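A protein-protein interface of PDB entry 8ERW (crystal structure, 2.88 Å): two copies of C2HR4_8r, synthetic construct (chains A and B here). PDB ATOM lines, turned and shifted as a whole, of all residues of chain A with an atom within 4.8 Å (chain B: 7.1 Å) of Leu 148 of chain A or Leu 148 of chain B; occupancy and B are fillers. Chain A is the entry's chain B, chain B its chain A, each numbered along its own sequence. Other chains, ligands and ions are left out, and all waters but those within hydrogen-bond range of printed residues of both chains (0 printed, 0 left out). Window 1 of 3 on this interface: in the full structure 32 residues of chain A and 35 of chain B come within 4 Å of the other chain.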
ATOM      1  N   GLU A 141      13.592  19.295  17.817  1.00  0.00           N
ATOM      2  CA  GLU A 141      13.212  18.092  17.084  1.00  0.00           C
ATOM      3  C   GLU A 141      14.392  17.140  16.923  1.00  0.00           C
ATOM      4  O   GLU A 141      14.235  15.920  17.061  1.00  0.00           O
ATOM      5  CB  GLU A 141      12.649  18.480  15.715  1.00  0.00           C
ATOM      6  CG  GLU A 141      11.858  17.384  15.024  1.00  0.00           C
ATOM      7  CD  GLU A 141      11.596  17.695  13.563  1.00  0.00           C
ATOM      8  OE1 GLU A 141      11.635  18.887  13.190  1.00  0.00           O
ATOM      9  OE2 GLU A 141      11.366  16.746  12.784  1.00  0.00           O
ATOM     10  N   ALA A 143      17.226  16.861  18.788  1.00  0.00           N
ATOM     11  CA  ALA A 143      17.696  16.274  20.038  1.00  0.00           C
ATOM     12  C   ALA A 143      16.803  15.120  20.480  1.00  0.00           C
ATOM     13  O   ALA A 143      17.301  14.067  20.893  1.00  0.00           O
ATOM     14  CB  ALA A 143      17.768  17.348  21.125  1.00  0.00           C
ATOM     15  N   LEU A 144      15.482  15.289  20.392  1.00  0.00           N
ATOM     16  CA  LEU A 144      14.581  14.209  20.784  1.00  0.00           C
ATOM     17  C   LEU A 144      14.811  12.967  19.930  1.00  0.00           C
ATOM     18  O   LEU A 144      14.960  11.856  20.452  1.00  0.00           O
ATOM     19  CB  LEU A 144      13.129  14.665  20.672  1.00  0.00           C
ATOM     20  CG  LEU A 144      12.612  15.571  21.784  1.00  0.00           C
ATOM     21  CD1 LEU A 144      11.350  16.286  21.341  1.00  0.00           C
ATOM     22  CD2 LEU A 144      12.346  14.769  23.044  1.00  0.00           C
ATOM     23  N   ALA A 145      14.825  13.136  18.605  1.00  0.00           N
ATOM     24  CA  ALA A 145      15.043  11.994  17.724  1.00  0.00           C
ATOM     25  C   ALA A 145      16.420  11.384  17.954  1.00  0.00           C
ATOM     26  O   ALA A 145      16.573  10.157  17.961  1.00  0.00           O
ATOM     27  CB  ALA A 145      14.879  12.416  16.265  1.00  0.00           C
ATOM     28  N   VAL A 146      17.435  12.228  18.142  1.00  0.00           N
ATOM     29  CA  VAL A 146      18.756  11.723  18.495  1.00  0.00           C
ATOM     30  C   VAL A 146      18.704  10.994  19.831  1.00  0.00           C
ATOM     31  O   VAL A 146      19.282   9.910  19.988  1.00  0.00           O
ATOM     32  CB  VAL A 146      19.775  12.877  18.520  1.00  0.00           C
ATOM     33  CG1 VAL A 146      21.030  12.456  19.262  1.00  0.00           C
ATOM     34  CG2 VAL A 146      20.106  13.318  17.104  1.00  0.00           C
ATOM     35  N   ALA A 147      18.014  11.576  20.816  1.00  0.00           N
ATOM     36  CA  ALA A 147      17.898  10.932  22.121  1.00  0.00           C
ATOM     37  C   ALA A 147      17.228   9.572  22.013  1.00  0.00           C
ATOM     38  O   ALA A 147      17.570   8.651  22.766  1.00  0.00           O
ATOM     39  CB  ALA A 147      17.118  11.834  23.080  1.00  0.00           C
ATOM     40  N   LEU A 148      16.280   9.424  21.090  1.00  0.00           N
ATOM     41  CA  LEU A 148      15.699   8.116  20.829  1.00  0.00           C
ATOM     42  C   LEU A 148      16.766   7.136  20.364  1.00  0.00           C
ATOM     43  O   LEU A 148      17.003   6.100  20.997  1.00  0.00           O
ATOM     44  CB  LEU A 148      14.600   8.237  19.779  1.00  0.00           C
ATOM     45  CG  LEU A 148      13.265   8.804  20.239  1.00  0.00           C
ATOM     46  CD1 LEU A 148      12.384   8.993  19.024  1.00  0.00           C
ATOM     47  CD2 LEU A 148      12.616   7.886  21.239  1.00  0.00           C
ATOM     48  N   VAL A 149      17.422   7.449  19.245  1.00  0.00           N
ATOM     49  CA  VAL A 149      18.456   6.566  18.716  1.00  0.00           C
ATOM     50  C   VAL A 149      19.498   6.258  19.776  1.00  0.00           C
ATOM     51  O   VAL A 149      20.038   5.145  19.822  1.00  0.00           O
ATOM     52  CB  VAL A 149      19.085   7.198  17.458  1.00  0.00           C
ATOM     53  CG1 VAL A 149      20.464   6.628  17.204  1.00  0.00           C
ATOM     54  CG2 VAL A 149      18.182   6.964  16.255  1.00  0.00           C
ATOM     55  N   LEU A 150      19.793   7.220  20.652  1.00  0.00           N
ATOM     56  CA  LEU A 150      20.725   6.960  21.743  1.00  0.00           C
ATOM     57  C   LEU A 150      20.115   6.011  22.766  1.00  0.00           C
ATOM     58  O   LEU A 150      20.760   5.048  23.199  1.00  0.00           O
ATOM     59  CB  LEU A 150      21.127   8.272  22.413  1.00  0.00           C
ATOM     60  CG  LEU A 150      22.214   9.087  21.717  1.00  0.00           C
ATOM     61  CD1 LEU A 150      22.271  10.485  22.312  1.00  0.00           C
ATOM     62  CD2 LEU A 150      23.558   8.393  21.842  1.00  0.00           C
ATOM     63  N   SER A 151      18.873   6.276  23.176  1.00  0.00           N
ATOM     64  CA  SER A 151      18.222   5.405  24.146  1.00  0.00           C
ATOM     65  C   SER A 151      18.180   3.964  23.656  1.00  0.00           C
ATOM     66  O   SER A 151      18.298   3.030  24.457  1.00  0.00           O
ATOM     67  CB  SER A 151      16.808   5.907  24.437  1.00  0.00           C
ATOM     68  OG  SER A 151      16.296   5.318  25.619  1.00  0.00           O
ATOM     69  N   LEU A 152      18.020   3.766  22.345  1.00  0.00           N
ATOM     70  CA  LEU A 152      17.964   2.419  21.790  1.00  0.00           C
ATOM     71  C   LEU A 152      19.349   1.792  21.700  1.00  0.00           C
ATOM     72  O   LEU A 152      19.521   0.614  22.034  1.00  0.00           O
ATOM     73  CB  LEU A 152      17.301   2.455  20.413  1.00  0.00           C
ATOM     74  CG  LEU A 152      15.779   2.600  20.443  1.00  0.00           C
ATOM     75  CD1 LEU A 152      15.267   3.425  19.275  1.00  0.00           C
ATOM     76  CD2 LEU A 152      15.128   1.218  20.450  1.00  0.00           C
ATOM     77  N   LEU A 178      15.032   9.456  13.161  1.00  0.00           N
ATOM     78  CA  LEU A 178      13.684   8.913  13.281  1.00  0.00           C
ATOM     79  C   LEU A 178      13.510   7.650  12.451  1.00  0.00           C
ATOM     80  O   LEU A 178      12.745   6.759  12.836  1.00  0.00           O
ATOM     81  CB  LEU A 178      12.659   9.967  12.867  1.00  0.00           C
ATOM     82  CG  LEU A 178      12.274  10.951  13.971  1.00  0.00           C
ATOM     83  CD1 LEU A 178      11.451  12.096  13.435  1.00  0.00           C
ATOM     84  CD2 LEU A 178      11.504  10.206  15.051  1.00  0.00           C
ATOM     85  N   ALA A 181      15.783   4.967  14.412  1.00  0.00           N
ATOM     86  CA  ALA A 181      15.100   4.597  15.647  1.00  0.00           C
ATOM     87  C   ALA A 181      13.957   3.632  15.369  1.00  0.00           C
ATOM     88  O   ALA A 181      13.738   2.678  16.126  1.00  0.00           O
ATOM     89  CB  ALA A 181      14.586   5.850  16.356  1.00  0.00           C
ATOM     90  N   GLU B 107      16.362   8.853  33.152  1.00  0.00           N
ATOM     91  CA  GLU B 107      15.896   8.807  31.773  1.00  0.00           C
ATOM     92  C   GLU B 107      14.373   8.802  31.709  1.00  0.00           C
ATOM     93  O   GLU B 107      13.772   9.554  30.931  1.00  0.00           O
ATOM     94  CB  GLU B 107      16.466   7.575  31.075  1.00  0.00           C
ATOM     95  CG  GLU B 107      16.079   7.442  29.615  1.00  0.00           C
ATOM     96  CD  GLU B 107      16.650   6.185  28.998  1.00  0.00           C
ATOM     97  OE1 GLU B 107      17.630   5.651  29.559  1.00  0.00           O
ATOM     98  OE2 GLU B 107      16.119   5.726  27.968  1.00  0.00           O
ATOM     99  N   VAL B 115       6.803  14.721  27.875  1.00  0.00           N
ATOM    100  CA  VAL B 115       5.414  14.424  27.537  1.00  0.00           C
ATOM    101  C   VAL B 115       4.470  15.211  28.431  1.00  0.00           C
ATOM    102  O   VAL B 115       3.475  15.779  27.961  1.00  0.00           O
ATOM    103  CB  VAL B 115       5.154  12.908  27.634  1.00  0.00           C
ATOM    104  CG1 VAL B 115       3.693  12.630  27.926  1.00  0.00           C
ATOM    105  CG2 VAL B 115       5.559  12.232  26.341  1.00  0.00           C
ATOM    106  N   LEU B 118       4.876  18.948  27.475  1.00  0.00           N
ATOM    107  CA  LEU B 118       4.293  19.213  26.166  1.00  0.00           C
ATOM    108  C   LEU B 118       2.776  19.078  26.203  1.00  0.00           C
ATOM    109  O   LEU B 118       2.064  19.826  25.524  1.00  0.00           O
ATOM    110  CB  LEU B 118       4.892  18.270  25.122  1.00  0.00           C
ATOM    111  CG  LEU B 118       6.345  18.552  24.741  1.00  0.00           C
ATOM    112  CD1 LEU B 118       6.937  17.398  23.944  1.00  0.00           C
ATOM    113  CD2 LEU B 118       6.448  19.846  23.948  1.00  0.00           C
ATOM    114  N   SER B 140      10.105   4.498  28.700  1.00  0.00           N
ATOM    115  CA  SER B 140      10.989   5.562  28.236  1.00  0.00           C
ATOM    116  C   SER B 140      10.856   5.782  26.734  1.00  0.00           C
ATOM    117  O   SER B 140      10.901   6.923  26.259  1.00  0.00           O
ATOM    118  CB  SER B 140      12.440   5.235  28.589  1.00  0.00           C
ATOM    119  OG  SER B 140      13.315   6.210  28.048  1.00  0.00           O
ATOM    120  N   GLU B 141      10.699   4.701  25.969  1.00  0.00           N
ATOM    121  CA  GLU B 141      10.652   4.829  24.515  1.00  0.00           C
ATOM    122  C   GLU B 141       9.340   5.450  24.051  1.00  0.00           C
ATOM    123  O   GLU B 141       9.328   6.251  23.110  1.00  0.00           O
ATOM    124  CB  GLU B 141      10.854   3.459  23.869  1.00  0.00           C
ATOM    125  CG  GLU B 141      10.954   3.486  22.355  1.00  0.00           C
ATOM    126  CD  GLU B 141      10.972   2.094  21.755  1.00  0.00           C
ATOM    127  OE1 GLU B 141      10.908   1.116  22.527  1.00  0.00           O
ATOM    128  OE2 GLU B 141      11.043   1.976  20.514  1.00  0.00           O
ATOM    129  N   VAL B 142       8.226   5.097  24.698  1.00  0.00           N
ATOM    130  CA  VAL B 142       6.930   5.629  24.289  1.00  0.00           C
ATOM    131  C   VAL B 142       6.822   7.109  24.635  1.00  0.00           C
ATOM    132  O   VAL B 142       6.313   7.912  23.843  1.00  0.00           O
ATOM    133  CB  VAL B 142       5.791   4.822  24.939  1.00  0.00           C
ATOM    134  CG1 VAL B 142       4.438   5.408  24.553  1.00  0.00           C
ATOM    135  CG2 VAL B 142       5.877   3.359  24.547  1.00  0.00           C
ATOM    136  N   ALA B 143       7.284   7.492  25.826  1.00  0.00           N
ATOM    137  CA  ALA B 143       7.216   8.894  26.225  1.00  0.00           C
ATOM    138  C   ALA B 143       7.964   9.785  25.240  1.00  0.00           C
ATOM    139  O   ALA B 143       7.473  10.854  24.865  1.00  0.00           O
ATOM    140  CB  ALA B 143       7.776   9.062  27.636  1.00  0.00           C
ATOM    141  N   LEU B 144       9.148   9.360  24.798  1.00  0.00           N
ATOM    142  CA  LEU B 144       9.907  10.164  23.845  1.00  0.00           C
ATOM    143  C   LEU B 144       9.201  10.235  22.496  1.00  0.00           C
ATOM    144  O   LEU B 144       9.042  11.319  21.921  1.00  0.00           O
ATOM    145  CB  LEU B 144      11.312   9.585  23.678  1.00  0.00           C
ATOM    146  CG  LEU B 144      12.396  10.206  24.551  1.00  0.00           C
ATOM    147  CD1 LEU B 144      13.559   9.261  24.730  1.00  0.00           C
ATOM    148  CD2 LEU B 144      12.865  11.505  23.921  1.00  0.00           C
ATOM    149  N   ALA B 145       8.785   9.083  21.964  1.00  0.00           N
ATOM    150  CA  ALA B 145       8.130   9.073  20.660  1.00  0.00           C
ATOM    151  C   ALA B 145       6.868   9.925  20.677  1.00  0.00           C
ATOM    152  O   ALA B 145       6.574  10.634  19.705  1.00  0.00           O
ATOM    153  CB  ALA B 145       7.807   7.638  20.247  1.00  0.00           C
ATOM    154  N   VAL B 146       6.108   9.869  21.773  1.00  0.00           N
ATOM    155  CA  VAL B 146       4.924  10.709  21.897  1.00  0.00           C
ATOM    156  C   VAL B 146       5.321  12.174  21.995  1.00  0.00           C
ATOM    157  O   VAL B 146       4.696  13.044  21.375  1.00  0.00           O
ATOM    158  CB  VAL B 146       4.092  10.279  23.120  1.00  0.00           C
ATOM    159  CG1 VAL B 146       2.926  11.237  23.317  1.00  0.00           C
ATOM    160  CG2 VAL B 146       3.603   8.854  22.966  1.00  0.00           C
ATOM    161  N   ALA B 147       6.351  12.473  22.790  1.00  0.00           N
ATOM    162  CA  ALA B 147       6.820  13.847  22.920  1.00  0.00           C
ATOM    163  C   ALA B 147       7.137  14.445  21.558  1.00  0.00           C
ATOM    164  O   ALA B 147       6.906  15.637  21.321  1.00  0.00           O
ATOM    165  CB  ALA B 147       8.051  13.895  23.826  1.00  0.00           C
ATOM    166  N   LEU B 148       7.677  13.634  20.650  1.00  0.00           N
ATOM    167  CA  LEU B 148       7.875  14.089  19.281  1.00  0.00           C
ATOM    168  C   LEU B 148       6.545  14.484  18.652  1.00  0.00           C
ATOM    169  O   LEU B 148       6.339  15.640  18.267  1.00  0.00           O
ATOM    170  CB  LEU B 148       8.555  12.994  18.462  1.00  0.00           C
ATOM    171  CG  LEU B 148       9.993  12.689  18.862  1.00  0.00           C
ATOM    172  CD1 LEU B 148      10.504  11.475  18.112  1.00  0.00           C
ATOM    173  CD2 LEU B 148      10.876  13.896  18.596  1.00  0.00           C
ATOM    174  N   VAL B 149       5.620  13.527  18.556  1.00  0.00           N
ATOM    175  CA  VAL B 149       4.324  13.809  17.946  1.00  0.00           C
ATOM    176  C   VAL B 149       3.673  15.013  18.611  1.00  0.00           C
ATOM    177  O   VAL B 149       3.042  15.845  17.945  1.00  0.00           O
ATOM    178  CB  VAL B 149       3.424  12.561  18.012  1.00  0.00           C
ATOM    179  CG1 VAL B 149       1.962  12.954  18.002  1.00  0.00           C
ATOM    180  CG2 VAL B 149       3.739  11.636  16.842  1.00  0.00           C
ATOM    181  N   LEU B 150       3.815  15.129  19.932  1.00  0.00           N
ATOM    182  CA  LEU B 150       3.285  16.296  20.629  1.00  0.00           C
ATOM    183  C   LEU B 150       4.025  17.562  20.218  1.00  0.00           C
ATOM    184  O   LEU B 150       3.406  18.570  19.857  1.00  0.00           O
ATOM    185  CB  LEU B 150       3.383  16.096  22.140  1.00  0.00           C
ATOM    186  CG  LEU B 150       2.322  15.207  22.783  1.00  0.00           C
ATOM    187  CD1 LEU B 150       2.763  14.784  24.174  1.00  0.00           C
ATOM    188  CD2 LEU B 150       0.992  15.940  22.841  1.00  0.00           C
ATOM    189  N   SER B 151       5.359  17.530  20.279  1.00  0.00           N
ATOM    190  CA  SER B 151       6.139  18.700  19.896  1.00  0.00           C
ATOM    191  C   SER B 151       5.794  19.143  18.481  1.00  0.00           C
ATOM    192  O   SER B 151       5.739  20.345  18.194  1.00  0.00           O
ATOM    193  CB  SER B 151       7.632  18.393  20.014  1.00  0.00           C
ATOM    194  OG  SER B 151       8.407  19.550  19.761  1.00  0.00           O
ATOM    195  N   LEU B 152       5.549  18.185  17.585  1.00  0.00           N
ATOM    196  CA  LEU B 152       5.236  18.522  16.201  1.00  0.00           C
ATOM    197  C   LEU B 152       3.811  19.037  16.056  1.00  0.00           C
ATOM    198  O   LEU B 152       3.555  19.948  15.260  1.00  0.00           O
ATOM    199  CB  LEU B 152       5.465  17.303  15.307  1.00  0.00           C
ATOM    200  CG  LEU B 152       6.916  17.140  14.853  1.00  0.00           C
ATOM    201  CD1 LEU B 152       7.299  15.683  14.675  1.00  0.00           C
ATOM    202  CD2 LEU B 152       7.135  17.911  13.553  1.00  0.00           C
ATOM    203  N   ALA B 153       2.870  18.474  16.816  1.00  0.00           N
ATOM    204  CA  ALA B 153       1.499  18.966  16.753  1.00  0.00           C
ATOM    205  C   ALA B 153       1.400  20.380  17.311  1.00  0.00           C
ATOM    206  O   ALA B 153       0.671  21.220  16.768  1.00  0.00           O
ATOM    207  CB  ALA B 153       0.566  18.020  17.511  1.00  0.00           C
ATOM    208  N   ASN B 154       2.127  20.667  18.394  1.00  0.00           N
ATOM    209  CA  ASN B 154       2.096  22.011  18.958  1.00  0.00           C
ATOM    210  C   ASN B 154       2.677  23.036  17.991  1.00  0.00           C
ATOM    211  O   ASN B 154       2.268  24.203  18.003  1.00  0.00           O
ATOM    212  CB  ASN B 154       2.855  22.050  20.286  1.00  0.00           C
ATOM    213  CG  ASN B 154       2.168  21.248  21.380  1.00  0.00           C
ATOM    214  OD1 ASN B 154       1.048  20.765  21.209  1.00  0.00           O
ATOM    215  ND2 ASN B 154       2.836  21.118  22.522  1.00  0.00           N
ATOM    216  N   ALA B 165      -2.485  13.826  18.115  1.00  0.00           N
ATOM    217  CA  ALA B 165      -1.364  13.474  18.976  1.00  0.00           C
ATOM    218  C   ALA B 165      -1.849  12.865  20.284  1.00  0.00           C
ATOM    219  O   ALA B 165      -1.229  11.935  20.815  1.00  0.00           O
ATOM    220  CB  ALA B 165      -0.504  14.709  19.247  1.00  0.00           C
ATOM    221  N   SER B 174       4.784   3.196  20.444  1.00  0.00           N
ATOM    222  CA  SER B 174       5.946   3.944  19.980  1.00  0.00           C
ATOM    223  C   SER B 174       6.074   3.888  18.463  1.00  0.00           C
ATOM    224  O   SER B 174       6.633   4.806  17.853  1.00  0.00           O
ATOM    225  CB  SER B 174       7.220   3.401  20.626  1.00  0.00           C
ATOM    226  OG  SER B 174       7.594   2.161  20.048  1.00  0.00           O
ATOM    227  N   ALA B 177       3.536   6.426  16.879  1.00  0.00           N
ATOM    228  CA  ALA B 177       4.030   7.763  17.185  1.00  0.00           C
ATOM    229  C   ALA B 177       5.262   8.095  16.353  1.00  0.00           C
ATOM    230  O   ALA B 177       5.405   9.218  15.856  1.00  0.00           O
ATOM    231  CB  ALA B 177       4.346   7.879  18.676  1.00  0.00           C
ATOM    232  N   LEU B 178       6.165   7.126  16.190  1.00  0.00           N
ATOM    233  CA  LEU B 178       7.379   7.375  15.420  1.00  0.00           C
ATOM    234  C   LEU B 178       7.078   7.468  13.932  1.00  0.00           C
ATOM    235  O   LEU B 178       7.715   8.243  13.210  1.00  0.00           O
ATOM    236  CB  LEU B 178       8.397   6.273  15.693  1.00  0.00           C
ATOM    237  CG  LEU B 178       9.281   6.526  16.911  1.00  0.00           C
ATOM    238  CD1 LEU B 178      10.009   5.273  17.321  1.00  0.00           C
ATOM    239  CD2 LEU B 178      10.270   7.634  16.586  1.00  0.00           C
ATOM    240  N   ALA B 181       5.127  11.005  13.715  1.00  0.00           N
ATOM    241  CA  ALA B 181       6.088  12.091  13.863  1.00  0.00           C
ATOM    242  C   ALA B 181       6.959  12.227  12.625  1.00  0.00           C
ATOM    243  O   ALA B 181       7.432  13.325  12.308  1.00  0.00           O
ATOM    244  CB  ALA B 181       6.958  11.860  15.099  1.00  0.00           C
ATOM    245  N   LEU B 182       7.176  11.124  11.909  1.00  0.00           N
ATOM    246  CA  LEU B 182       7.981  11.173  10.698  1.00  0.00           C
ATOM    247  C   LEU B 182       7.264  11.927   9.589  1.00  0.00           C
ATOM    248  O   LEU B 182       7.857  12.780   8.919  1.00  0.00           O
ATOM    249  CB  LEU B 182       8.312   9.757  10.248  1.00  0.00           C
ATOM    250  CG  LEU B 182       9.794   9.405  10.285  1.00  0.00           C
ATOM    251  CD1 LEU B 182       9.913   7.899  10.187  1.00  0.00           C
ATOM    252  CD2 LEU B 182      10.540  10.096   9.170  1.00  0.00           C
ATOM    253  N   LEU B 184       4.593  14.027   9.868  1.00  0.00           N
ATOM    254  CA  LEU B 184       4.448  15.408  10.316  1.00  0.00           C
ATOM    255  C   LEU B 184       5.744  16.183  10.115  1.00  0.00           C
ATOM    256  O   LEU B 184       5.750  17.284   9.555  1.00  0.00           O
ATOM    257  CB  LEU B 184       4.038  15.442  11.787  1.00  0.00           C
ATOM    258  CG  LEU B 184       2.613  15.010  12.123  1.00  0.00           C
ATOM    259  CD1 LEU B 184       2.388  15.056  13.626  1.00  0.00           C
ATOM    260  CD2 LEU B 184       1.610  15.893  11.411  1.00  0.00           C
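The side-chain carboxylate (OE2) of Glu 107 of chain B sits at hydrogen-bond distance from the side-chain hydroxyl (OG) of Ser 140 of chain B (2.8 Å).
Among the printed residues, merely in contact across the chains: Leu 144 of chain A with Leu 148 of chain B (3.2 Å), Leu 178 of chain A with Leu 178 of chain B (3.2 Å), Leu 148 of chain A with Leu 148 of chain B (3.2 Å), Leu 148 of chain A with Leu 144 of chain B (3.2 Å), Leu 144 of chain A with Leu 144 of chain B (3.4 Å), Leu 178 of chain A with Leu 148 of chain B (3.5 Å), Leu 148 of chain A with Leu 178 of chain B (3.5 Å), Leu 178 of chain A with Leu 182 of chain B (3.9 Å) and Ser 151 of chain A with Ser 140 of chain B (3.9 Å).
OG of Ser 151 of chain A sits close to OE2 of Glu 107 of chain B (2.4 Å).
Of the printed residues of chain B, Leu 178 of chain A touches Leu 148, Leu 178 and Leu 182.
Of the printed residues of chain A, Glu 107 of chain B touches Ser 151.
Of the printed residues of chain A, Leu 148 of chain B touches Leu 144 (3.2 Å), Leu 148 (3.2 Å) and Leu 178 (3.5 Å).
The nearest residue of chain A that does not touch Leu 148 of chain B is Ala 145 of chain A (4.02 Å).
The nearest printed residue of chain A that does not touch Leu 178 of chain B is Ala 181 of chain A (4.7 Å).
Leu 144 of chain A touches Leu 148 of chain B, and with the chains exchanged Leu 148 of chain A touches Leu 144 of chain B.
Leu 148 of chain B touches its own counterpart, Leu 148 of chain A.
Leu 148 of chain A touches Leu 178 of chain B, and with the chains exchanged Leu 178 of chain A touches Leu 148 of chain B.
Leu 178 of chain B touches its own counterpart, Leu 178 of chain A.
Positions printed for both chains: 141, 143, 144, 145, 146, 147, 148, 149, 150, 151, 152, 178 and 181.
Of the 10 pairs that touch across the chains among the printed residues, 7 have their exchanged pair printed and touching as well.
Of the 13 printed residues of chain A, 4 touch a printed residue of chain B.
Printed residues of chain A that touch a printed residue of chain B: Leu 144, Leu 148, Ser 151 and Leu 178.
Hydrophobic or aromatic side chains of chain B within 4 Å of the printed part of chain A: Leu 144, Leu 148, Leu 178 and Leu 182.
Among the printed residues, 10 pairs touch across the chains.
Among the printed residues, no Asp or Glu carboxylate lies within 4 Å of a Lys or Arg side-chain nitrogen of the other chain.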
